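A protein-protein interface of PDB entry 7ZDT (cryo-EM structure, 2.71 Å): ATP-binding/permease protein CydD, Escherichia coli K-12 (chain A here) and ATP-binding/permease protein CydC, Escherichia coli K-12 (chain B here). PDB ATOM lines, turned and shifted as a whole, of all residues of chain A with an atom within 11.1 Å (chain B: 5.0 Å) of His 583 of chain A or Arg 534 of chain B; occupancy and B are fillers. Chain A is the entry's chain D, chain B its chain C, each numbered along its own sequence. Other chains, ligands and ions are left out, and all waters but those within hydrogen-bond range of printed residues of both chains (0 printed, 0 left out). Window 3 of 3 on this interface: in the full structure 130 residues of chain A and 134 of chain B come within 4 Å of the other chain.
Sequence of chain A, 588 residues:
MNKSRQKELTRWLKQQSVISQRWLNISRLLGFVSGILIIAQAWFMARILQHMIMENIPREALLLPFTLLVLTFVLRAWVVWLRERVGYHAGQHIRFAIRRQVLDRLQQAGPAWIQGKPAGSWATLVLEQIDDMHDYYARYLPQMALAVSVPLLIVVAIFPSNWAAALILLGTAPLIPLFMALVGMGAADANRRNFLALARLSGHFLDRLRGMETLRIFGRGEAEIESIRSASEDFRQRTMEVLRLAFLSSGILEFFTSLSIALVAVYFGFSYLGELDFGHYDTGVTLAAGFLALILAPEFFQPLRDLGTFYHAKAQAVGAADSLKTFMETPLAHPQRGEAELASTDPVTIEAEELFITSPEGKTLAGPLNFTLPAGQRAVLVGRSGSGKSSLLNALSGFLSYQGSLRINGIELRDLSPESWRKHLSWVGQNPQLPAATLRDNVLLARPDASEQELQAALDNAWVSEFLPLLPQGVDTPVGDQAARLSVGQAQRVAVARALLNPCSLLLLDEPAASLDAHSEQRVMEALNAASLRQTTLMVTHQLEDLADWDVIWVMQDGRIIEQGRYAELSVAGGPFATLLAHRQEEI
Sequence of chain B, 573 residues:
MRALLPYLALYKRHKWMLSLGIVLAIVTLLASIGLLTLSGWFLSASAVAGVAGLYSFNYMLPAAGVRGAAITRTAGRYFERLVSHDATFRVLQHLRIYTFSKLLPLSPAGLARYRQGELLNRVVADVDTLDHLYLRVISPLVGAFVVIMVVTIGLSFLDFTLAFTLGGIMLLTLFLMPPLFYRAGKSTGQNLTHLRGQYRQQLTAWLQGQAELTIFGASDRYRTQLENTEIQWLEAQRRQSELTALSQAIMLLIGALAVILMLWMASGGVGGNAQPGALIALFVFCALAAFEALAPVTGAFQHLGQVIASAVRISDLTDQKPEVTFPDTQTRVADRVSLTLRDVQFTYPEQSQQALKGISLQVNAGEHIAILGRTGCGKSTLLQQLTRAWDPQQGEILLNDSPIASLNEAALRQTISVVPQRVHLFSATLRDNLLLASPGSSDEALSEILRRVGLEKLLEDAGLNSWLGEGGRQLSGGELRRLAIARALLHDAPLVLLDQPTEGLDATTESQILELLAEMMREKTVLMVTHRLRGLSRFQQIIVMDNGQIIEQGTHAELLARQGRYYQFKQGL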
ATOM      1  N   GLY A 383      -6.467 -24.044  26.010  1.00  0.00           N
ATOM      2  CA  GLY A 383      -6.026 -22.692  25.725  1.00  0.00           C
ATOM      3  C   GLY A 383      -7.004 -21.965  24.827  1.00  0.00           C
ATOM      4  O   GLY A 383      -8.048 -22.501  24.482  1.00  0.00           O
ATOM      5  N   ARG A 384      -6.663 -20.740  24.451  1.00  0.00           N
ATOM      6  CA  ARG A 384      -7.509 -19.919  23.591  1.00  0.00           C
ATOM      7  C   ARG A 384      -7.535 -20.437  22.164  1.00  0.00           C
ATOM      8  O   ARG A 384      -6.619 -21.114  21.739  1.00  0.00           O
ATOM      9  CB  ARG A 384      -7.002 -18.480  23.586  1.00  0.00           C
ATOM     10  CG  ARG A 384      -7.268 -17.711  24.866  1.00  0.00           C
ATOM     11  CD  ARG A 384      -8.495 -16.830  24.730  1.00  0.00           C
ATOM     12  NE  ARG A 384      -8.502 -15.772  25.734  1.00  0.00           N
ATOM     13  CZ  ARG A 384      -7.660 -14.743  25.735  1.00  0.00           C
ATOM     14  NH1 ARG A 384      -7.732 -13.820  26.687  1.00  0.00           N
ATOM     15  NH2 ARG A 384      -6.737 -14.638  24.789  1.00  0.00           N
ATOM     16  N   ALA A 518     -25.015 -32.866  25.548  1.00  0.00           N
ATOM     17  CA  ALA A 518     -24.499 -33.109  26.890  1.00  0.00           C
ATOM     18  C   ALA A 518     -24.430 -34.598  27.207  1.00  0.00           C
ATOM     19  O   ALA A 518     -23.485 -35.056  27.858  1.00  0.00           O
ATOM     20  CB  ALA A 518     -25.356 -32.379  27.921  1.00  0.00           C
ATOM     21  N   HIS A 542     -11.862 -28.269  24.902  1.00  0.00           N
ATOM     22  CA  HIS A 542     -12.335 -27.055  25.549  1.00  0.00           C
ATOM     23  C   HIS A 542     -13.086 -27.341  26.840  1.00  0.00           C
ATOM     24  O   HIS A 542     -13.242 -26.435  27.663  1.00  0.00           O
ATOM     25  CB  HIS A 542     -13.239 -26.259  24.602  1.00  0.00           C
ATOM     26  CG  HIS A 542     -14.392 -27.048  24.065  1.00  0.00           C
ATOM     27  ND1 HIS A 542     -14.243 -28.024  23.103  1.00  0.00           N
ATOM     28  CD2 HIS A 542     -15.712 -27.016  24.366  1.00  0.00           C
ATOM     29  CE1 HIS A 542     -15.422 -28.553  22.828  1.00  0.00           C
ATOM     30  NE2 HIS A 542     -16.330 -27.959  23.582  1.00  0.00           N
ATOM     31  N   GLN A 543     -13.559 -28.571  27.025  1.00  0.00           N
ATOM     32  CA  GLN A 543     -14.140 -28.964  28.300  1.00  0.00           C
ATOM     33  C   GLN A 543     -13.075 -28.939  29.385  1.00  0.00           C
ATOM     34  O   GLN A 543     -11.950 -29.402  29.183  1.00  0.00           O
ATOM     35  CB  GLN A 543     -14.756 -30.356  28.200  1.00  0.00           C
ATOM     36  CG  GLN A 543     -16.237 -30.344  27.902  1.00  0.00           C
ATOM     37  CD  GLN A 543     -16.535 -29.811  26.521  1.00  0.00           C
ATOM     38  OE1 GLN A 543     -16.043 -30.335  25.522  1.00  0.00           O
ATOM     39  NE2 GLN A 543     -17.341 -28.759  26.454  1.00  0.00           N
ATOM     40  N   LEU A 544     -13.418 -28.389  30.552  1.00  0.00           N
ATOM     41  CA  LEU A 544     -12.407 -28.254  31.635  1.00  0.00           C
ATOM     42  C   LEU A 544     -12.887 -28.926  32.926  1.00  0.00           C
ATOM     43  O   LEU A 544     -12.080 -29.631  33.557  1.00  0.00           O
ATOM     44  CB  LEU A 544     -12.157 -26.760  31.853  1.00  0.00           C
ATOM     45  CG  LEU A 544     -11.790 -25.980  30.593  1.00  0.00           C
ATOM     46  CD1 LEU A 544     -12.087 -24.499  30.762  1.00  0.00           C
ATOM     47  CD2 LEU A 544     -10.331 -26.196  30.224  1.00  0.00           C
ATOM     48  N   GLU A 545     -14.159 -28.739  33.283  1.00  0.00           N
ATOM     49  CA  GLU A 545     -14.713 -29.314  34.538  1.00  0.00           C
ATOM     50  C   GLU A 545     -14.639 -30.845  34.497  1.00  0.00           C
ATOM     51  O   GLU A 545     -14.280 -31.445  35.528  1.00  0.00           O
ATOM     52  CB  GLU A 545     -16.157 -28.848  34.736  1.00  0.00           C
ATOM     53  CG  GLU A 545     -17.015 -28.969  33.490  1.00  0.00           C
ATOM     54  CD  GLU A 545     -16.711 -27.940  32.413  1.00  0.00           C
ATOM     55  OE1 GLU A 545     -15.639 -27.312  32.488  1.00  0.00           O
ATOM     56  OE2 GLU A 545     -17.550 -27.769  31.506  1.00  0.00           O
ATOM     57  N   TYR A 567      -5.018 -30.968  37.654  1.00  0.00           N
ATOM     58  CA  TYR A 567      -6.173 -30.085  37.780  1.00  0.00           C
ATOM     59  C   TYR A 567      -6.217 -29.411  39.146  1.00  0.00           C
ATOM     60  O   TYR A 567      -6.544 -28.224  39.247  1.00  0.00           O
ATOM     61  CB  TYR A 567      -7.457 -30.869  37.528  1.00  0.00           C
ATOM     62  CG  TYR A 567      -8.714 -30.038  37.632  1.00  0.00           C
ATOM     63  CD1 TYR A 567      -9.152 -29.270  36.565  1.00  0.00           C
ATOM     64  CD2 TYR A 567      -9.468 -30.028  38.798  1.00  0.00           C
ATOM     65  CE1 TYR A 567     -10.300 -28.511  36.653  1.00  0.00           C
ATOM     66  CE2 TYR A 567     -10.617 -29.272  38.897  1.00  0.00           C
ATOM     67  CZ  TYR A 567     -11.029 -28.516  37.822  1.00  0.00           C
ATOM     68  OH  TYR A 567     -12.174 -27.761  37.918  1.00  0.00           O
ATOM     69  N   SER A 571      -6.189 -25.315  39.067  1.00  0.00           N
ATOM     70  CA  SER A 571      -7.504 -24.699  39.213  1.00  0.00           C
ATOM     71  C   SER A 571      -7.490 -23.582  40.251  1.00  0.00           C
ATOM     72  O   SER A 571      -8.136 -22.545  40.064  1.00  0.00           O
ATOM     73  CB  SER A 571      -8.541 -25.758  39.585  1.00  0.00           C
ATOM     74  OG  SER A 571      -8.263 -26.319  40.855  1.00  0.00           O
ATOM     75  N   GLY A 575      -3.577 -17.837  37.392  1.00  0.00           N
ATOM     76  CA  GLY A 575      -3.006 -17.977  36.076  1.00  0.00           C
ATOM     77  C   GLY A 575      -4.070 -17.963  35.000  1.00  0.00           C
ATOM     78  O   GLY A 575      -5.191 -17.487  35.210  1.00  0.00           O
ATOM     79  N   PRO A 576      -3.742 -18.490  33.819  1.00  0.00           N
ATOM     80  CA  PRO A 576      -4.725 -18.494  32.731  1.00  0.00           C
ATOM     81  C   PRO A 576      -5.711 -19.644  32.796  1.00  0.00           C
ATOM     82  O   PRO A 576      -6.836 -19.495  32.308  1.00  0.00           O
ATOM     83  CB  PRO A 576      -3.842 -18.566  31.477  1.00  0.00           C
ATOM     84  CG  PRO A 576      -2.463 -19.023  31.975  1.00  0.00           C
ATOM     85  CD  PRO A 576      -2.552 -19.265  33.449  1.00  0.00           C
ATOM     86  N   PHE A 577      -5.335 -20.784  33.378  1.00  0.00           N
ATOM     87  CA  PHE A 577      -6.268 -21.904  33.457  1.00  0.00           C
ATOM     88  C   PHE A 577      -7.455 -21.570  34.350  1.00  0.00           C
ATOM     89  O   PHE A 577      -8.605 -21.850  33.997  1.00  0.00           O
ATOM     90  CB  PHE A 577      -5.558 -23.157  33.964  1.00  0.00           C
ATOM     91  CG  PHE A 577      -6.457 -24.354  34.061  1.00  0.00           C
ATOM     92  CD1 PHE A 577      -6.728 -24.937  35.285  1.00  0.00           C
ATOM     93  CD2 PHE A 577      -7.038 -24.891  32.927  1.00  0.00           C
ATOM     94  CE1 PHE A 577      -7.557 -26.036  35.374  1.00  0.00           C
ATOM     95  CE2 PHE A 577      -7.869 -25.988  33.012  1.00  0.00           C
ATOM     96  CZ  PHE A 577      -8.128 -26.561  34.238  1.00  0.00           C
ATOM     97  N   ALA A 578      -7.194 -20.980  35.517  1.00  0.00           N
ATOM     98  CA  ALA A 578      -8.288 -20.568  36.390  1.00  0.00           C
ATOM     99  C   ALA A 578      -9.143 -19.501  35.721  1.00  0.00           C
ATOM    100  O   ALA A 578     -10.375 -19.526  35.823  1.00  0.00           O
ATOM    101  CB  ALA A 578      -7.740 -20.064  37.722  1.00  0.00           C
ATOM    102  N   THR A 579      -8.505 -18.551  35.036  1.00  0.00           N
ATOM    103  CA  THR A 579      -9.254 -17.596  34.226  1.00  0.00           C
ATOM    104  C   THR A 579     -10.020 -18.310  33.121  1.00  0.00           C
ATOM    105  O   THR A 579     -11.177 -17.977  32.839  1.00  0.00           O
ATOM    106  CB  THR A 579      -8.304 -16.554  33.634  1.00  0.00           C
ATOM    107  OG1 THR A 579      -7.590 -15.902  34.691  1.00  0.00           O
ATOM    108  CG2 THR A 579      -9.080 -15.518  32.838  1.00  0.00           C
ATOM    109  N   LEU A 580      -9.386 -19.298  32.486  1.00  0.00           N
ATOM    110  CA  LEU A 580     -10.068 -20.103  31.479  1.00  0.00           C
ATOM    111  C   LEU A 580     -11.226 -20.881  32.092  1.00  0.00           C
ATOM    112  O   LEU A 580     -12.301 -20.987  31.493  1.00  0.00           O
ATOM    113  CB  LEU A 580      -9.068 -21.052  30.821  1.00  0.00           C
ATOM    114  CG  LEU A 580      -9.262 -21.450  29.363  1.00  0.00           C
ATOM    115  CD1 LEU A 580      -9.423 -20.220  28.489  1.00  0.00           C
ATOM    116  CD2 LEU A 580      -8.076 -22.275  28.912  1.00  0.00           C
ATOM    117  N   LEU A 581     -11.018 -21.436  33.286  1.00  0.00           N
ATOM    118  CA  LEU A 581     -12.050 -22.197  33.976  1.00  0.00           C
ATOM    119  C   LEU A 581     -13.136 -21.311  34.577  1.00  0.00           C
ATOM    120  O   LEU A 581     -14.243 -21.797  34.829  1.00  0.00           O
ATOM    121  CB  LEU A 581     -11.411 -23.051  35.074  1.00  0.00           C
ATOM    122  CG  LEU A 581     -12.290 -23.989  35.900  1.00  0.00           C
ATOM    123  CD1 LEU A 581     -12.925 -25.047  35.019  1.00  0.00           C
ATOM    124  CD2 LEU A 581     -11.475 -24.631  37.007  1.00  0.00           C
ATOM    125  N   ALA A 582     -12.847 -20.027  34.799  1.00  0.00           N
ATOM    126  CA  ALA A 582     -13.814 -19.148  35.450  1.00  0.00           C
ATOM    127  C   ALA A 582     -15.073 -18.984  34.611  1.00  0.00           C
ATOM    128  O   ALA A 582     -16.184 -18.922  35.152  1.00  0.00           O
ATOM    129  CB  ALA A 582     -13.177 -17.789  35.732  1.00  0.00           C
ATOM    130  N   HIS A 583     -14.924 -18.902  33.288  1.00  0.00           N
ATOM    131  CA  HIS A 583     -16.086 -18.704  32.428  1.00  0.00           C
ATOM    132  C   HIS A 583     -16.966 -19.947  32.377  1.00  0.00           C
ATOM    133  O   HIS A 583     -18.197 -19.842  32.311  1.00  0.00           O
ATOM    134  CB  HIS A 583     -15.636 -18.297  31.027  1.00  0.00           C
ATOM    135  CG  HIS A 583     -14.903 -16.992  30.988  1.00  0.00           C
ATOM    136  ND1 HIS A 583     -13.533 -16.905  31.090  1.00  0.00           N
ATOM    137  CD2 HIS A 583     -15.352 -15.722  30.862  1.00  0.00           C
ATOM    138  CE1 HIS A 583     -13.168 -15.637  31.028  1.00  0.00           C
ATOM    139  NE2 HIS A 583     -14.252 -14.899  30.888  1.00  0.00           N
ATOM    140  N   ALA B 507     -13.764 -21.200  26.474  1.00  0.00           N
ATOM    141  CA  ALA B 507     -14.761 -20.567  27.330  1.00  0.00           C
ATOM    142  C   ALA B 507     -14.727 -19.049  27.205  1.00  0.00           C
ATOM    143  O   ALA B 507     -15.779 -18.402  27.155  1.00  0.00           O
ATOM    144  CB  ALA B 507     -14.542 -20.985  28.781  1.00  0.00           C
ATOM    145  N   THR B 508     -13.532 -18.460  27.161  1.00  0.00           N
ATOM    146  CA  THR B 508     -13.436 -17.006  27.092  1.00  0.00           C
ATOM    147  C   THR B 508     -13.876 -16.497  25.726  1.00  0.00           C
ATOM    148  O   THR B 508     -14.606 -15.505  25.626  1.00  0.00           O
ATOM    149  CB  THR B 508     -12.009 -16.554  27.398  1.00  0.00           C
ATOM    150  OG1 THR B 508     -11.669 -16.918  28.740  1.00  0.00           O
ATOM    151  CG2 THR B 508     -11.903 -15.045  27.271  1.00  0.00           C
ATOM    152  N   GLU B 510     -15.918 -18.006  23.646  1.00  0.00           N
ATOM    153  CA  GLU B 510     -17.358 -18.207  23.532  1.00  0.00           C
ATOM    154  C   GLU B 510     -18.124 -17.096  24.238  1.00  0.00           C
ATOM    155  O   GLU B 510     -19.140 -16.614  23.729  1.00  0.00           O
ATOM    156  CB  GLU B 510     -17.744 -19.571  24.097  1.00  0.00           C
ATOM    157  CG  GLU B 510     -19.238 -19.801  24.171  1.00  0.00           C
ATOM    158  CD  GLU B 510     -19.597 -21.078  24.896  1.00  0.00           C
ATOM    159  OE1 GLU B 510     -18.687 -21.721  25.457  1.00  0.00           O
ATOM    160  OE2 GLU B 510     -20.790 -21.442  24.903  1.00  0.00           O
ATOM    161  N   SER B 511     -17.649 -16.677  25.412  1.00  0.00           N
ATOM    162  CA  SER B 511     -18.306 -15.594  26.134  1.00  0.00           C
ATOM    163  C   SER B 511     -18.268 -14.298  25.337  1.00  0.00           C
ATOM    164  O   SER B 511     -19.256 -13.558  25.294  1.00  0.00           O
ATOM    165  CB  SER B 511     -17.642 -15.392  27.494  1.00  0.00           C
ATOM    166  OG  SER B 511     -16.342 -14.851  27.347  1.00  0.00           O
ATOM    167  N   LEU B 514     -20.771 -14.760  22.403  1.00  0.00           N
ATOM    168  CA  LEU B 514     -22.154 -14.704  22.865  1.00  0.00           C
ATOM    169  C   LEU B 514     -22.538 -13.302  23.309  1.00  0.00           C
ATOM    170  O   LEU B 514     -23.691 -12.891  23.139  1.00  0.00           O
ATOM    171  CB  LEU B 514     -22.373 -15.702  24.000  1.00  0.00           C
ATOM    172  CG  LEU B 514     -22.312 -17.179  23.610  1.00  0.00           C
ATOM    173  CD1 LEU B 514     -22.601 -18.069  24.804  1.00  0.00           C
ATOM    174  CD2 LEU B 514     -23.275 -17.470  22.477  1.00  0.00           C
ATOM    175  N   ARG B 532     -24.953 -26.524  24.052  1.00  0.00           N
ATOM    176  CA  ARG B 532     -24.467 -25.979  25.346  1.00  0.00           C
ATOM    177  C   ARG B 532     -25.609 -25.233  26.039  1.00  0.00           C
ATOM    178  O   ARG B 532     -26.035 -24.197  25.505  1.00  0.00           O
ATOM    179  CB  ARG B 532     -23.294 -25.026  25.093  1.00  0.00           C
ATOM    180  CG  ARG B 532     -22.296 -25.537  24.064  1.00  0.00           C
ATOM    181  CD  ARG B 532     -21.007 -24.741  24.000  1.00  0.00           C
ATOM    182  NE  ARG B 532     -19.971 -25.494  23.306  1.00  0.00           N
ATOM    183  CZ  ARG B 532     -18.747 -25.049  23.050  1.00  0.00           C
ATOM    184  NH1 ARG B 532     -18.386 -23.835  23.428  1.00  0.00           N
ATOM    185  NH2 ARG B 532     -17.886 -25.822  22.414  1.00  0.00           N
ATOM    186  N   LEU B 533     -26.049 -25.732  27.199  1.00  0.00           N
ATOM    187  CA  LEU B 533     -27.139 -25.090  27.984  1.00  0.00           C
ATOM    188  C   LEU B 533     -26.539 -23.973  28.846  1.00  0.00           C
ATOM    189  O   LEU B 533     -26.628 -24.065  30.087  1.00  0.00           O
ATOM    190  CB  LEU B 533     -27.819 -26.152  28.855  1.00  0.00           C
ATOM    191  CG  LEU B 533     -28.424 -27.334  28.100  1.00  0.00           C
ATOM    192  CD1 LEU B 533     -27.345 -28.128  27.382  1.00  0.00           C
ATOM    193  CD2 LEU B 533     -29.208 -28.235  29.043  1.00  0.00           C
ATOM    194  N   ARG B 534     -25.957 -22.960  28.196  1.00  0.00           N
ATOM    195  CA  ARG B 534     -25.317 -21.806  28.878  1.00  0.00           C
ATOM    196  C   ARG B 534     -26.006 -20.517  28.424  1.00  0.00           C
ATOM    197  O   ARG B 534     -26.170 -20.336  27.203  1.00  0.00           O
ATOM    198  CB  ARG B 534     -23.840 -21.731  28.487  1.00  0.00           C
ATOM    199  CG  ARG B 534     -23.242 -20.340  28.632  1.00  0.00           C
ATOM    200  CD  ARG B 534     -22.078 -20.106  27.694  1.00  0.00           C
ATOM    201  NE  ARG B 534     -21.539 -18.766  27.859  1.00  0.00           N
ATOM    202  CZ  ARG B 534     -20.591 -18.441  28.728  1.00  0.00           C
ATOM    203  NH1 ARG B 534     -20.166 -17.193  28.806  1.00  0.00           N
ATOM    204  NH2 ARG B 534     -20.073 -19.363  29.519  1.00  0.00           N
ATOM    205  N   GLY B 535     -26.352 -19.641  29.370  1.00  0.00           N
ATOM    206  CA  GLY B 535     -27.020 -18.371  29.032  1.00  0.00           C
ATOM    207  C   GLY B 535     -28.315 -18.592  28.270  1.00  0.00           C
ATOM    208  O   GLY B 535     -28.548 -17.869  27.282  1.00  0.00           O
ATOM    209  N   LEU B 536     -29.106 -19.588  28.686  1.00  0.00           N
ATOM    210  CA  LEU B 536     -30.417 -19.890  28.049  1.00  0.00           C
ATOM    211  C   LEU B 536     -31.512 -19.038  28.702  1.00  0.00           C
ATOM    212  O   LEU B 536     -32.658 -19.070  28.215  1.00  0.00           O
ATOM    213  CB  LEU B 536     -30.718 -21.387  28.188  1.00  0.00           C
ATOM    214  CG  LEU B 536     -30.367 -22.246  26.974  1.00  0.00           C
ATOM    215  CD1 LEU B 536     -29.013 -21.857  26.404  1.00  0.00           C
ATOM    216  CD2 LEU B 536     -30.389 -23.721  27.334  1.00  0.00           C
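The guanidinium group (NH2) of Arg 534 of chain B lies within hydrogen-bond range of the backbone carbonyl oxygen (O) of His 583 of chain A (3.4 Å).
NH2 of Arg 532 of chain B sits at hydrogen-bond distance from NE2 of His 542 of chain A (2.9 Å).
The side-chain hydroxyl (OG1) of Thr 508 of chain B is in hydrogen-bond range of a ring nitrogen (ND1) of His 583 of chain A, 3.0 Å away.
CG2 of Thr 508 of chain B touches NE of Arg 384 of chain A (3.8 Å).
Leu 580 of chain A touches Ala 507 of chain B.
His 583 of chain A touches Ala 507 of chain B.
Ser 511 of chain B touches His 583 of chain A (OG to CD2, 3.8 Å).
Hydrophobic or aromatic side chains of chain B within 4 Å of the printed part of chain A: Ala 507.
Among the printed residues, no Asp or Glu carboxylate lies within 4 Å of a Lys or Arg side-chain nitrogen of the other chain.
Of chain B, only Ala 507, Thr 508, Ser 511 and Arg 534 come within 4 Å of His 583 of chain A.
Arg 534 of chain B touches just one residue of chain A: His 583.
Of chain A, only Leu 580 and His 583 come within 4 Å of Ala 507 of chain B.
Glu 510 of chain B touches none of the printed residues of chain A.
Ser 511 of chain B touches one residue of chain A.
No residue of chain A comes within 4 Å of Leu 533 of chain B.
No residue of chain A comes within 4 Å of Leu 536 of chain B.
Printed residues of chain B within 4 Å of His 542 of chain A: Arg 532.
Of the printed residues of chain A, Thr 508 of chain B touches Arg 384 (3.8 Å) and His 583 (3.0 Å).
Printed residues of chain B within 4 Å of Arg 384 of chain A: Thr 508 (3.8 Å).
The nearest residue of chain A that does not touch Arg 534 of chain B is Ala 582 of chain A (6.9 Å).
The backbone carbonyl oxygen (O) of Thr 508 of chain B sits at hydrogen-bond distance from the side-chain hydroxyl (OG) of Ser 511 of chain B (2.5 Å).
OE1 of Gln 543 of chain A lies within hydrogen-bond range of NE2 of His 542 of chain A (3.1 Å).
OE1 of Glu 510 of chain B is in salt-bridge range of NH1 of Arg 532 of chain B, 2.9 Å away.
The backbone carbonyl oxygen (O) of Thr 579 of chain A sits at hydrogen-bond distance from a ring nitrogen (ND1) of His 583 of chain A (3.1 Å).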
